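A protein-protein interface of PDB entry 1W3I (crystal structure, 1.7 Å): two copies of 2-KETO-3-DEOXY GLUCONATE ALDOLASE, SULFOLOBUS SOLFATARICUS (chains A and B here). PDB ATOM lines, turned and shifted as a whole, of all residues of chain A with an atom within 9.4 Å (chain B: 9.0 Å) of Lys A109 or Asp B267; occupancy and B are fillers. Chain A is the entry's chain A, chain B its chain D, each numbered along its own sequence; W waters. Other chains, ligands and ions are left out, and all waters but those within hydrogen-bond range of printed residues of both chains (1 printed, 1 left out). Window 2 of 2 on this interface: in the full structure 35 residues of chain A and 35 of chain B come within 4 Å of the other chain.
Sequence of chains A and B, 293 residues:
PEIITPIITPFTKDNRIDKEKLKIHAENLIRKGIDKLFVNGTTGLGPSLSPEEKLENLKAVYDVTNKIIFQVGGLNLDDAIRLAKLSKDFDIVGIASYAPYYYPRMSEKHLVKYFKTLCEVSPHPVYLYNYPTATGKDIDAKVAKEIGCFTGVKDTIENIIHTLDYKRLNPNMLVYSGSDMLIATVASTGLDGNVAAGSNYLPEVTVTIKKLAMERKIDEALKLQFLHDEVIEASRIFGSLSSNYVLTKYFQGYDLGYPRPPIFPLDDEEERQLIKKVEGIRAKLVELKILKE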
ATOM      1  N   ARG A 105      -2.095   4.550  -6.730  1.00  0.00           N
ATOM      2  CA  ARG A 105      -2.232   3.709  -7.935  1.00  0.00           C
ATOM      3  C   ARG A 105      -2.570   4.497  -9.218  1.00  0.00           C
ATOM      4  O   ARG A 105      -3.555   4.195  -9.951  1.00  0.00           O
ATOM      5  CB  ARG A 105      -3.244   2.584  -7.689  1.00  0.00           C
ATOM      6  CG  ARG A 105      -2.776   1.622  -6.563  1.00  0.00           C
ATOM      7  CD  ARG A 105      -3.066   0.150  -6.817  1.00  0.00           C
ATOM      8  NE  ARG A 105      -4.422  -0.184  -6.371  1.00  0.00           N
ATOM      9  CZ  ARG A 105      -5.389  -0.667  -7.155  1.00  0.00           C
ATOM     10  NH1 ARG A 105      -6.584  -0.934  -6.625  1.00  0.00           N
ATOM     11  NH2 ARG A 105      -5.169  -0.884  -8.459  1.00  0.00           N
ATOM     12  N   MET A 106      -1.754   5.507  -9.491  1.00  0.00           N
ATOM     13  CA  MET A 106      -1.803   6.231 -10.764  1.00  0.00           C
ATOM     14  C   MET A 106      -0.847   5.500 -11.706  1.00  0.00           C
ATOM     15  O   MET A 106       0.254   5.179 -11.299  1.00  0.00           O
ATOM     16  CB  MET A 106      -1.344   7.685 -10.561  1.00  0.00           C
ATOM     17  CG  MET A 106      -2.242   8.538  -9.658  1.00  0.00           C
ATOM     18  SD  MET A 106      -1.605  10.220  -9.505  1.00  0.00           S
ATOM     19  CE  MET A 106      -1.752  10.779 -11.240  1.00  0.00           C
ATOM     20  N   SER A 107      -1.244   5.241 -12.959  1.00  0.00           N
ATOM     21  CA  SER A 107      -0.423   4.412 -13.866  1.00  0.00           C
ATOM     22  C   SER A 107       0.933   5.071 -14.155  1.00  0.00           C
ATOM     23  O   SER A 107       1.048   6.294 -14.129  1.00  0.00           O
ATOM     24  CB  SER A 107      -1.158   4.170 -15.186  1.00  0.00           C
ATOM     25  OG  SER A 107      -1.326   5.402 -15.879  1.00  0.00           O
ATOM     26  N   GLU A 108       1.947   4.263 -14.422  1.00  0.00           N
ATOM     27  CA  GLU A 108       3.227   4.759 -14.886  1.00  0.00           C
ATOM     28  C   GLU A 108       3.019   5.637 -16.121  1.00  0.00           C
ATOM     29  O   GLU A 108       3.620   6.692 -16.241  1.00  0.00           O
ATOM     30  CB  GLU A 108       4.166   3.619 -15.222  1.00  0.00           C
ATOM     31  CG  GLU A 108       5.580   4.092 -15.520  1.00  0.00           C
ATOM     32  CD  GLU A 108       6.550   2.985 -15.893  1.00  0.00           C
ATOM     33  OE1 GLU A 108       7.289   3.168 -16.882  1.00  0.00           O
ATOM     34  OE2 GLU A 108       6.596   1.952 -15.200  1.00  0.00           O
ATOM     35  N   LYS A 109       2.153   5.185 -17.026  1.00  0.00           N
ATOM     36  CA  LYS A 109       1.848   5.968 -18.218  1.00  0.00           C
ATOM     37  C   LYS A 109       1.412   7.397 -17.858  1.00  0.00           C
ATOM     38  O   LYS A 109       1.894   8.382 -18.447  1.00  0.00           O
ATOM     39  CB  LYS A 109       0.774   5.220 -19.027  1.00  0.00           C
ATOM     40  CG  LYS A 109       0.216   5.965 -20.214  1.00  0.00           C
ATOM     41  CD  LYS A 109      -0.374   4.904 -21.167  1.00  0.00           C
ATOM     42  CE  LYS A 109      -1.082   5.504 -22.389  1.00  0.00           C
ATOM     43  NZ  LYS A 109      -2.305   6.283 -21.989  1.00  0.00           N
ATOM     44  N   HIS A 110       0.503   7.531 -16.885  1.00  0.00           N
ATOM     45  CA  HIS A 110       0.019   8.860 -16.499  1.00  0.00           C
ATOM     46  C   HIS A 110       1.106   9.674 -15.784  1.00  0.00           C
ATOM     47  O   HIS A 110       1.203  10.887 -15.969  1.00  0.00           O
ATOM     48  CB  HIS A 110      -1.213   8.746 -15.609  1.00  0.00           C
ATOM     49  CG  HIS A 110      -2.468   8.383 -16.352  1.00  0.00           C
ATOM     50  ND1 HIS A 110      -2.517   8.242 -17.726  1.00  0.00           N
ATOM     51  CD2 HIS A 110      -3.720   8.139 -15.908  1.00  0.00           C
ATOM     52  CE1 HIS A 110      -3.754   7.921 -18.090  1.00  0.00           C
ATOM     53  NE2 HIS A 110      -4.498   7.856 -17.003  1.00  0.00           N
ATOM     54  N   LEU A 111       1.914   8.997 -14.973  1.00  0.00           N
ATOM     55  CA  LEU A 111       3.010   9.695 -14.265  1.00  0.00           C
ATOM     56  C   LEU A 111       4.035  10.231 -15.266  1.00  0.00           C
ATOM     57  O   LEU A 111       4.497  11.368 -15.159  1.00  0.00           O
ATOM     58  CB  LEU A 111       3.698   8.746 -13.286  1.00  0.00           C
ATOM     59  CG  LEU A 111       2.812   8.365 -12.088  1.00  0.00           C
ATOM     60  CD1 LEU A 111       3.322   7.158 -11.354  1.00  0.00           C
ATOM     61  CD2 LEU A 111       2.641   9.568 -11.178  1.00  0.00           C
ATOM     62  N   VAL A 112       4.390   9.399 -16.237  1.00  0.00           N
ATOM     63  CA  VAL A 112       5.369   9.774 -17.247  1.00  0.00           C
ATOM     64  C   VAL A 112       4.782  10.954 -18.024  1.00  0.00           C
ATOM     65  O   VAL A 112       5.492  11.905 -18.320  1.00  0.00           O
ATOM     66  CB  VAL A 112       5.718   8.553 -18.186  1.00  0.00           C
ATOM     67  CG1 VAL A 112       6.402   9.038 -19.452  1.00  0.00           C
ATOM     68  CG2 VAL A 112       6.623   7.514 -17.439  1.00  0.00           C
ATOM     69  N   LYS A 113       3.479  10.926 -18.317  1.00  0.00           N
ATOM     70  CA  LYS A 113       2.868  12.022 -19.077  1.00  0.00           C
ATOM     71  C   LYS A 113       2.897  13.335 -18.318  1.00  0.00           C
ATOM     72  O   LYS A 113       3.176  14.402 -18.893  1.00  0.00           O
ATOM     73  CB  LYS A 113       1.429  11.691 -19.507  1.00  0.00           C
ATOM     74  CG  LYS A 113       0.806  12.657 -20.566  1.00  0.00           C
ATOM     75  CD  LYS A 113      -0.643  12.176 -20.893  1.00  0.00           C
ATOM     76  CE  LYS A 113      -1.281  12.857 -22.133  1.00  0.00           C
ATOM     77  NZ  LYS A 113      -0.509  14.024 -22.530  1.00  0.00           N
ATOM     78  N   TYR A 114       2.614  13.276 -17.014  1.00  0.00           N
ATOM     79  CA  TYR A 114       2.718  14.469 -16.181  1.00  0.00           C
ATOM     80  C   TYR A 114       4.112  15.131 -16.288  1.00  0.00           C
ATOM     81  O   TYR A 114       4.240  16.334 -16.504  1.00  0.00           O
ATOM     82  CB  TYR A 114       2.420  14.097 -14.720  1.00  0.00           C
ATOM     83  CG  TYR A 114       2.703  15.216 -13.728  1.00  0.00           C
ATOM     84  CD1 TYR A 114       1.736  16.193 -13.456  1.00  0.00           C
ATOM     85  CD2 TYR A 114       3.939  15.287 -13.050  1.00  0.00           C
ATOM     86  CE1 TYR A 114       1.993  17.237 -12.553  1.00  0.00           C
ATOM     87  CE2 TYR A 114       4.206  16.334 -12.150  1.00  0.00           C
ATOM     88  CZ  TYR A 114       3.240  17.289 -11.918  1.00  0.00           C
ATOM     89  OH  TYR A 114       3.498  18.289 -11.040  1.00  0.00           O
ATOM     90  N   PHE A 115       5.152  14.327 -16.153  1.00  0.00           N
ATOM     91  CA  PHE A 115       6.501  14.878 -16.106  1.00  0.00           C
ATOM     92  C   PHE A 115       6.940  15.326 -17.512  1.00  0.00           C
ATOM     93  O   PHE A 115       7.583  16.378 -17.634  1.00  0.00           O
ATOM     94  CB  PHE A 115       7.484  13.869 -15.521  1.00  0.00           C
ATOM     95  CG  PHE A 115       7.443  13.804 -13.999  1.00  0.00           C
ATOM     96  CD1 PHE A 115       6.890  12.682 -13.346  1.00  0.00           C
ATOM     97  CD2 PHE A 115       7.968  14.851 -13.240  1.00  0.00           C
ATOM     98  CE1 PHE A 115       6.825  12.627 -11.986  1.00  0.00           C
ATOM     99  CE2 PHE A 115       7.917  14.825 -11.823  1.00  0.00           C
ATOM    100  CZ  PHE A 115       7.367  13.697 -11.194  1.00  0.00           C
ATOM    101  N   LYS A 116       6.610  14.537 -18.545  1.00  0.00           N
ATOM    102  CA  LYS A 116       6.991  14.955 -19.915  1.00  0.00           C
ATOM    103  C   LYS A 116       6.334  16.263 -20.324  1.00  0.00           C
ATOM    104  O   LYS A 116       6.963  17.088 -21.002  1.00  0.00           O
ATOM    105  CB  LYS A 116       6.728  13.858 -20.958  1.00  0.00           C
ATOM    106  CG  LYS A 116       7.841  12.807 -21.019  1.00  0.00           C
ATOM    107  CD  LYS A 116       7.450  11.717 -22.040  1.00  0.00           C
ATOM    108  CE  LYS A 116       8.573  10.729 -22.263  1.00  0.00           C
ATOM    109  NZ  LYS A 116       8.411  10.035 -23.579  1.00  0.00           N
ATOM    110  N   THR A 117       5.108  16.491 -19.852  1.00  0.00           N
ATOM    111  CA  THR A 117       4.393  17.751 -20.072  1.00  0.00           C
ATOM    112  C   THR A 117       5.104  18.965 -19.488  1.00  0.00           C
ATOM    113  O   THR A 117       5.258  20.004 -20.163  1.00  0.00           O
ATOM    114  CB  THR A 117       2.956  17.668 -19.516  1.00  0.00           C
ATOM    115  OG1 THR A 117       2.263  16.575 -20.128  1.00  0.00           O
ATOM    116  CG2 THR A 117       2.114  18.932 -19.942  1.00  0.00           C
ATOM    117  N   ILE A 139       9.164   7.351  -8.648  1.00  0.00           N
ATOM    118  CA  ILE A 139       9.695   7.600  -9.968  1.00  0.00           C
ATOM    119  C   ILE A 139      11.168   7.207  -9.922  1.00  0.00           C
ATOM    120  O   ILE A 139      12.070   8.048  -9.661  1.00  0.00           O
ATOM    121  CB  ILE A 139       9.527   9.073 -10.353  1.00  0.00           C
ATOM    122  CG1 ILE A 139       8.101   9.553 -10.000  1.00  0.00           C
ATOM    123  CG2 ILE A 139       9.962   9.290 -11.850  1.00  0.00           C
ATOM    124  CD1 ILE A 139       6.961   8.882 -10.793  1.00  0.00           C
ATOM    125  N   VAL A 143      12.061   4.705 -14.519  1.00  0.00           N
ATOM    126  CA  VAL A 143      11.010   5.621 -14.968  1.00  0.00           C
ATOM    127  C   VAL A 143      11.628   6.984 -15.289  1.00  0.00           C
ATOM    128  O   VAL A 143      11.238   7.631 -16.261  1.00  0.00           O
ATOM    129  CB  VAL A 143       9.872   5.761 -13.933  1.00  0.00           C
ATOM    130  CG1 VAL A 143       8.750   6.640 -14.484  1.00  0.00           C
ATOM    131  CG2 VAL A 143       9.337   4.385 -13.545  1.00  0.00           C
ATOM    132  N   GLU A 146      13.002   6.698 -18.702  1.00  0.00           N
ATOM    133  CA  GLU A 146      11.943   6.719 -19.716  1.00  0.00           C
ATOM    134  C   GLU A 146      11.401   8.142 -19.954  1.00  0.00           C
ATOM    135  O   GLU A 146      11.092   8.527 -21.099  1.00  0.00           O
ATOM    136  CB  GLU A 146      10.798   5.783 -19.331  1.00  0.00           C
ATOM    137  CG  GLU A 146       9.590   5.888 -20.256  1.00  0.00           C
ATOM    138  CD  GLU A 146       8.431   5.007 -19.817  1.00  0.00           C
ATOM    139  OE1 GLU A 146       8.469   4.480 -18.680  1.00  0.00           O
ATOM    140  OE2 GLU A 146       7.473   4.849 -20.613  1.00  0.00           O
ATOM    141  N   ILE A 147      11.289   8.928 -18.882  1.00  0.00           N
ATOM    142  CA  ILE A 147      10.864  10.316 -19.007  1.00  0.00           C
ATOM    143  C   ILE A 147      11.914  11.091 -19.808  1.00  0.00           C
ATOM    144  O   ILE A 147      11.566  11.890 -20.684  1.00  0.00           O
ATOM    145  CB  ILE A 147      10.604  10.932 -17.601  1.00  0.00           C
ATOM    146  CG1 ILE A 147       9.322  10.382 -17.009  1.00  0.00           C
ATOM    147  CG2 ILE A 147      10.510  12.453 -17.666  1.00  0.00           C
ATOM    148  CD1 ILE A 147       9.306  10.466 -15.475  1.00  0.00           C
ATOM    149  N   ILE B 237      -7.796  -1.339 -14.003  1.00  0.00           N
ATOM    150  CA  ILE B 237      -6.753  -1.698 -14.979  1.00  0.00           C
ATOM    151  C   ILE B 237      -5.998  -0.480 -15.492  1.00  0.00           C
ATOM    152  O   ILE B 237      -4.764  -0.454 -15.470  1.00  0.00           O
ATOM    153  CB  ILE B 237      -7.330  -2.493 -16.194  1.00  0.00           C
ATOM    154  CG1 ILE B 237      -7.920  -3.828 -15.712  1.00  0.00           C
ATOM    155  CG2 ILE B 237      -6.232  -2.737 -17.257  1.00  0.00           C
ATOM    156  CD1 ILE B 237      -8.959  -4.406 -16.703  1.00  0.00           C
ATOM    157  N   PHE B 238      -6.737   0.551 -15.910  1.00  0.00           N
ATOM    158  CA  PHE B 238      -6.116   1.758 -16.441  1.00  0.00           C
ATOM    159  C   PHE B 238      -6.155   2.965 -15.493  1.00  0.00           C
ATOM    160  O   PHE B 238      -5.659   4.080 -15.833  1.00  0.00           O
ATOM    161  CB  PHE B 238      -6.758   2.091 -17.814  1.00  0.00           C
ATOM    162  CG  PHE B 238      -6.593   0.993 -18.815  1.00  0.00           C
ATOM    163  CD1 PHE B 238      -7.687   0.226 -19.222  1.00  0.00           C
ATOM    164  CD2 PHE B 238      -5.308   0.662 -19.276  1.00  0.00           C
ATOM    165  CE1 PHE B 238      -7.516  -0.847 -20.135  1.00  0.00           C
ATOM    166  CE2 PHE B 238      -5.129  -0.393 -20.177  1.00  0.00           C
ATOM    167  CZ  PHE B 238      -6.221  -1.151 -20.595  1.00  0.00           C
ATOM    168  N   SER B 242     -10.036   7.753 -13.634  1.00  0.00           N
ATOM    169  CA  SER B 242     -10.280   8.053 -15.052  1.00  0.00           C
ATOM    170  C   SER B 242     -11.355   7.147 -15.629  1.00  0.00           C
ATOM    171  O   SER B 242     -12.243   7.590 -16.417  1.00  0.00           O
ATOM    172  CB  SER B 242      -8.974   7.845 -15.838  1.00  0.00           C
ATOM    173  OG  SER B 242      -7.991   8.755 -15.392  1.00  0.00           O
ATOM    174  N   SER B 243     -11.272   5.861 -15.283  1.00  0.00           N
ATOM    175  CA  SER B 243     -12.209   4.860 -15.863  1.00  0.00           C
ATOM    176  C   SER B 243     -13.656   5.131 -15.433  1.00  0.00           C
ATOM    177  O   SER B 243     -14.609   4.795 -16.175  1.00  0.00           O
ATOM    178  CB  SER B 243     -11.777   3.450 -15.470  1.00  0.00           C
ATOM    179  OG  SER B 243     -10.465   3.157 -15.965  1.00  0.00           O
ATOM    180  N   VAL B 246     -15.613   6.928 -18.061  1.00  0.00           N
ATOM    181  CA  VAL B 246     -15.964   6.073 -19.195  1.00  0.00           C
ATOM    182  C   VAL B 246     -17.121   5.150 -18.833  1.00  0.00           C
ATOM    183  O   VAL B 246     -18.116   5.013 -19.571  1.00  0.00           O
ATOM    184  CB  VAL B 246     -14.748   5.266 -19.700  1.00  0.00           C
ATOM    185  CG1 VAL B 246     -15.226   4.202 -20.748  1.00  0.00           C
ATOM    186  CG2 VAL B 246     -13.645   6.187 -20.232  1.00  0.00           C
ATOM    187  N   PRO B 262      -3.297  15.863 -13.548  1.00  0.00           N
ATOM    188  CA  PRO B 262      -2.758  14.580 -14.021  1.00  0.00           C
ATOM    189  C   PRO B 262      -3.626  13.326 -13.894  1.00  0.00           C
ATOM    190  O   PRO B 262      -3.125  12.220 -14.075  1.00  0.00           O
ATOM    191  CB  PRO B 262      -1.485  14.428 -13.166  1.00  0.00           C
ATOM    192  CG  PRO B 262      -1.906  15.061 -11.825  1.00  0.00           C
ATOM    193  CD  PRO B 262      -2.753  16.272 -12.240  1.00  0.00           C
ATOM    194  N   PHE B 264      -5.564  11.775 -16.098  1.00  0.00           N
ATOM    195  CA  PHE B 264      -5.763  11.931 -17.553  1.00  0.00           C
ATOM    196  C   PHE B 264      -6.893  11.011 -18.015  1.00  0.00           C
ATOM    197  O   PHE B 264      -7.048   9.931 -17.505  1.00  0.00           O
ATOM    198  CB  PHE B 264      -4.470  11.542 -18.273  1.00  0.00           C
ATOM    199  CG  PHE B 264      -3.343  12.521 -18.089  1.00  0.00           C
ATOM    200  CD1 PHE B 264      -2.288  12.217 -17.212  1.00  0.00           C
ATOM    201  CD2 PHE B 264      -3.335  13.738 -18.757  1.00  0.00           C
ATOM    202  CE1 PHE B 264      -1.218  13.107 -17.031  1.00  0.00           C
ATOM    203  CE2 PHE B 264      -2.237  14.659 -18.589  1.00  0.00           C
ATOM    204  CZ  PHE B 264      -1.187  14.328 -17.698  1.00  0.00           C
ATOM    205  N   PRO B 265      -7.686  11.435 -19.000  1.00  0.00           N
ATOM    206  CA  PRO B 265      -8.758  10.582 -19.525  1.00  0.00           C
ATOM    207  C   PRO B 265      -8.179   9.367 -20.218  1.00  0.00           C
ATOM    208  O   PRO B 265      -7.057   9.387 -20.767  1.00  0.00           O
ATOM    209  CB  PRO B 265      -9.494  11.501 -20.525  1.00  0.00           C
ATOM    210  CG  PRO B 265      -8.523  12.511 -20.898  1.00  0.00           C
ATOM    211  CD  PRO B 265      -7.552  12.704 -19.719  1.00  0.00           C
ATOM    212  N   LEU B 266      -8.937   8.274 -20.216  1.00  0.00           N
ATOM    213  CA  LEU B 266      -8.493   7.101 -20.935  1.00  0.00           C
ATOM    214  C   LEU B 266      -8.386   7.428 -22.431  1.00  0.00           C
ATOM    215  O   LEU B 266      -9.226   8.184 -22.941  1.00  0.00           O
ATOM    216  CB  LEU B 266      -9.491   5.963 -20.783  1.00  0.00           C
ATOM    217  CG  LEU B 266      -9.660   5.352 -19.370  1.00  0.00           C
ATOM    218  CD1 LEU B 266     -10.278   3.979 -19.536  1.00  0.00           C
ATOM    219  CD2 LEU B 266      -8.369   5.280 -18.606  1.00  0.00           C
ATOM    220  N   ASP B 267      -7.422   6.807 -23.097  1.00  0.00           N
ATOM    221  CA  ASP B 267      -7.303   6.962 -24.556  1.00  0.00           C
ATOM    222  C   ASP B 267      -8.185   5.930 -25.240  1.00  0.00           C
ATOM    223  O   ASP B 267      -8.816   5.119 -24.594  1.00  0.00           O
ATOM    224  CB  ASP B 267      -5.839   6.948 -25.040  1.00  0.00           C
ATOM    225  CG  ASP B 267      -5.138   5.634 -24.825  1.00  0.00           C
ATOM    226  OD1 ASP B 267      -5.761   4.551 -24.844  1.00  0.00           O
ATOM    227  OD2 ASP B 267      -3.912   5.611 -24.603  1.00  0.00           O
ATOM    228  N   ASP B 268      -8.290   5.988 -26.568  1.00  0.00           N
ATOM    229  CA  ASP B 268      -9.241   5.129 -27.259  1.00  0.00           C
ATOM    230  C   ASP B 268      -8.936   3.643 -27.060  1.00  0.00           C
ATOM    231  O   ASP B 268      -9.849   2.823 -26.935  1.00  0.00           O
ATOM    232  CB  ASP B 268      -9.179   5.435 -28.778  1.00  0.00           C
ATOM    233  CG  ASP B 268     -10.187   4.616 -29.558  1.00  0.00           C
ATOM    234  OD1 ASP B 268      -9.802   3.673 -30.295  1.00  0.00           O
ATOM    235  OD2 ASP B 268     -11.403   4.806 -29.432  1.00  0.00           O
ATOM    236  N   GLU B 269      -7.647   3.291 -27.073  1.00  0.00           N
ATOM    237  CA  GLU B 269      -7.270   1.879 -26.925  1.00  0.00           C
ATOM    238  C   GLU B 269      -7.661   1.396 -25.531  1.00  0.00           C
ATOM    239  O   GLU B 269      -8.237   0.310 -25.383  1.00  0.00           O
ATOM    240  CB  GLU B 269      -5.787   1.666 -27.159  1.00  0.00           C
ATOM    241  CG  GLU B 269      -5.305   0.219 -26.941  1.00  0.00           C
ATOM    242  CD  GLU B 269      -6.124  -0.867 -27.656  1.00  0.00           C
ATOM    243  OE1 GLU B 269      -6.842  -0.610 -28.648  1.00  0.00           O
ATOM    244  OE2 GLU B 269      -6.021  -2.040 -27.224  1.00  0.00           O
ATOM    245  N   GLU B 270      -7.406   2.228 -24.536  1.00  0.00           N
ATOM    246  CA  GLU B 270      -7.810   1.867 -23.159  1.00  0.00           C
ATOM    247  C   GLU B 270      -9.312   1.784 -22.999  1.00  0.00           C
ATOM    248  O   GLU B 270      -9.828   0.867 -22.371  1.00  0.00           O
ATOM    249  CB  GLU B 270      -7.257   2.880 -22.158  1.00  0.00           C
ATOM    250  CG  GLU B 270      -5.734   2.890 -22.118  1.00  0.00           C
ATOM    251  CD  GLU B 270      -5.183   4.091 -21.377  1.00  0.00           C
ATOM    252  OE1 GLU B 270      -5.824   5.156 -21.389  1.00  0.00           O
ATOM    253  OE2 GLU B 270      -4.093   3.973 -20.747  1.00  0.00           O
ATOM    254  N   GLU B 271     -10.046   2.732 -23.582  1.00  0.00           N
ATOM    255  CA  GLU B 271     -11.494   2.646 -23.536  1.00  0.00           C
ATOM    256  C   GLU B 271     -11.987   1.332 -24.195  1.00  0.00           C
ATOM    257  O   GLU B 271     -12.851   0.626 -23.659  1.00  0.00           O
ATOM    258  CB  GLU B 271     -12.069   3.901 -24.217  1.00  0.00           C
ATOM    259  CG  GLU B 271     -13.558   4.071 -24.149  1.00  0.00           C
ATOM    260  CD  GLU B 271     -13.978   5.472 -24.624  1.00  0.00           C
ATOM    261  OE1 GLU B 271     -15.026   5.550 -25.282  1.00  0.00           O
ATOM    262  OE2 GLU B 271     -13.273   6.488 -24.333  1.00  0.00           O
ATOM    263  N   ARG B 272     -11.431   0.982 -25.357  1.00  0.00           N
ATOM    264  CA  ARG B 272     -11.870  -0.256 -26.008  1.00  0.00           C
ATOM    265  C   ARG B 272     -11.650  -1.476 -25.127  1.00  0.00           C
ATOM    266  O   ARG B 272     -12.510  -2.355 -25.084  1.00  0.00           O
ATOM    267  CB  ARG B 272     -11.151  -0.484 -27.353  1.00  0.00           C
ATOM    268  CG  ARG B 272     -11.475   0.568 -28.392  1.00  0.00           C
ATOM    269  CD  ARG B 272     -10.709   0.307 -29.728  1.00  0.00           C
ATOM    270  NE  ARG B 272     -11.126   1.267 -30.756  1.00  0.00           N
ATOM    271  CZ  ARG B 272     -12.188   1.120 -31.557  1.00  0.00           C
ATOM    272  NH1 ARG B 272     -12.961   0.035 -31.506  1.00  0.00           N
ATOM    273  NH2 ARG B 272     -12.473   2.086 -32.420  1.00  0.00           N
ATOM    274  N   GLN B 273     -10.491  -1.543 -24.472  1.00  0.00           N
ATOM    275  CA  GLN B 273     -10.140  -2.695 -23.593  1.00  0.00           C
ATOM    276  C   GLN B 273     -11.052  -2.764 -22.377  1.00  0.00           C
ATOM    277  O   GLN B 273     -11.510  -3.865 -21.982  1.00  0.00           O
ATOM    278  CB  GLN B 273      -8.663  -2.653 -23.157  1.00  0.00           C
ATOM    279  CG  GLN B 273      -7.695  -3.024 -24.327  1.00  0.00           C
ATOM    280  CD  GLN B 273      -6.227  -3.210 -23.922  1.00  0.00           C
ATOM    281  OE1 GLN B 273      -5.912  -3.761 -22.858  1.00  0.00           O
ATOM    282  NE2 GLN B 273      -5.318  -2.772 -24.798  1.00  0.00           N
ATOM    283  N   LEU B 274     -11.341  -1.588 -21.819  1.00  0.00           N
ATOM    284  CA  LEU B 274     -12.259  -1.474 -20.691  1.00  0.00           C
ATOM    285  C   LEU B 274     -13.650  -1.959 -21.041  1.00  0.00           C
ATOM    286  O   LEU B 274     -14.238  -2.775 -20.323  1.00  0.00           O
ATOM    287  CB  LEU B 274     -12.276  -0.055 -20.128  1.00  0.00           C
ATOM    288  CG  LEU B 274     -13.245   0.181 -18.965  1.00  0.00           C
ATOM    289  CD1 LEU B 274     -12.951  -0.776 -17.762  1.00  0.00           C
ATOM    290  CD2 LEU B 274     -13.116   1.586 -18.519  1.00  0.00           C
ATOM    291  N   ILE B 275     -14.175  -1.477 -22.162  1.00  0.00           N
ATOM    292  CA  ILE B 275     -15.478  -1.936 -22.621  1.00  0.00           C
ATOM    293  C   ILE B 275     -15.505  -3.461 -22.840  1.00  0.00           C
ATOM    294  O   ILE B 275     -16.439  -4.139 -22.410  1.00  0.00           O
ATOM    295  CB  ILE B 275     -15.887  -1.139 -23.879  1.00  0.00           C
ATOM    296  CG1 ILE B 275     -16.213   0.304 -23.485  1.00  0.00           C
ATOM    297  CG2 ILE B 275     -17.063  -1.829 -24.601  1.00  0.00           C
ATOM    298  CD1 ILE B 275     -15.926   1.335 -24.566  1.00  0.00           C
HETATM  299  O   HOH W   1      -3.354   4.381 -17.724  1.00  0.00           O
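A ring nitrogen (NE2) of His A110 is in hydrogen-bond range of the backbone carbonyl oxygen (O) of Phe B264 (3.3 Å). OE2 of Glu B270 lies within salt-bridge range of NZ of Lys A109 (3.2 Å). The side-chain carboxylate of Asp B267 lies within salt-bridge range of the side-chain amino group of Lys A109.
OG of Ser A107 is in hydrogen-bond range of N of His A110 (3.0 Å). The backbone NH (N) of Asp B267 lies within hydrogen-bond range of the side-chain carboxylate (OE1) of Glu B270, at 2.9 Å. OD1 of Asp B267 sits at hydrogen-bond distance from N of Glu B269 (3.2 Å). OG1 of Thr A117 lies within hydrogen-bond range of O of Lys A113, at 2.7 Å. OG of Ser B242 is in hydrogen-bond range of O of Phe B264, 2.6 Å away.
Met A106 touches Pro B262 (CE to O, 3.5 Å). His A110 touches Ser B242. Phe B264 touches Lys A113 (CE2 to CD, 3.7 Å). CB of Pro B262 touches CD1 of Tyr A114 (3.7 Å). N of Tyr A114 touches CE1 of Phe B264, 3.8 Å away.
Of chain B, only Asp B267 (3.1 Å) and Glu B270 (3.2 Å) come within 4 Å of Lys A109. Of chain A, only Lys A109 comes within 4 Å of Asp B267. Glu B270 touches just one residue of chain A: Lys A109 (3.2 Å). Of the printed residues of chain B, His A110 touches Ser B242 (3.95 Å) and Phe B264 (3.3 Å). Printed residues of chain A within 4 Å of Ser B242: His A110. Of the printed residues of chain B, Met A106 touches Pro B262 (3.5 Å). Printed residues of chain B within 4 Å of Lys A113: Phe B264 (3.7 Å). Printed residues of chain A within 4 Å of Pro B262: Met A106 and Tyr A114. Ile B237 touches none of the printed residues of chain A. Ile B275 touches none of the printed residues of chain A. The nearest printed residue of chain B that does not touch Lys A109 is Pro B265 (5.8 Å). The nearest residue of chain A that does not touch Asp B267 is His A110 (6.3 Å). The nearest printed residue of chain A that does not touch Phe B264 is Thr A117 (4.8 Å).
Of the 17 printed residues of chain A, 5 touch a printed residue of chain B. Of the 18 printed residues of chain B, 5 touch a printed residue of chain A. Among the printed residues, Asp or Glu carboxylates within 4 Å of a Lys or Arg side-chain nitrogen of the other chain: Lys A109 with Asp B267 and Lys A109 with Glu B270.
No position is printed for both chains. Of the 8 pairs that touch across the chains among the printed residues, none has its exchanged pair printed and touching as well.
Water W1 lies within hydrogen-bond range of the side-chain hydroxyl of Ser A107 (2.9 Å), the backbone carbonyl oxygen of Phe B238 (3.0 Å) and the side-chain carboxylate of Glu B270 (3.1 Å).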
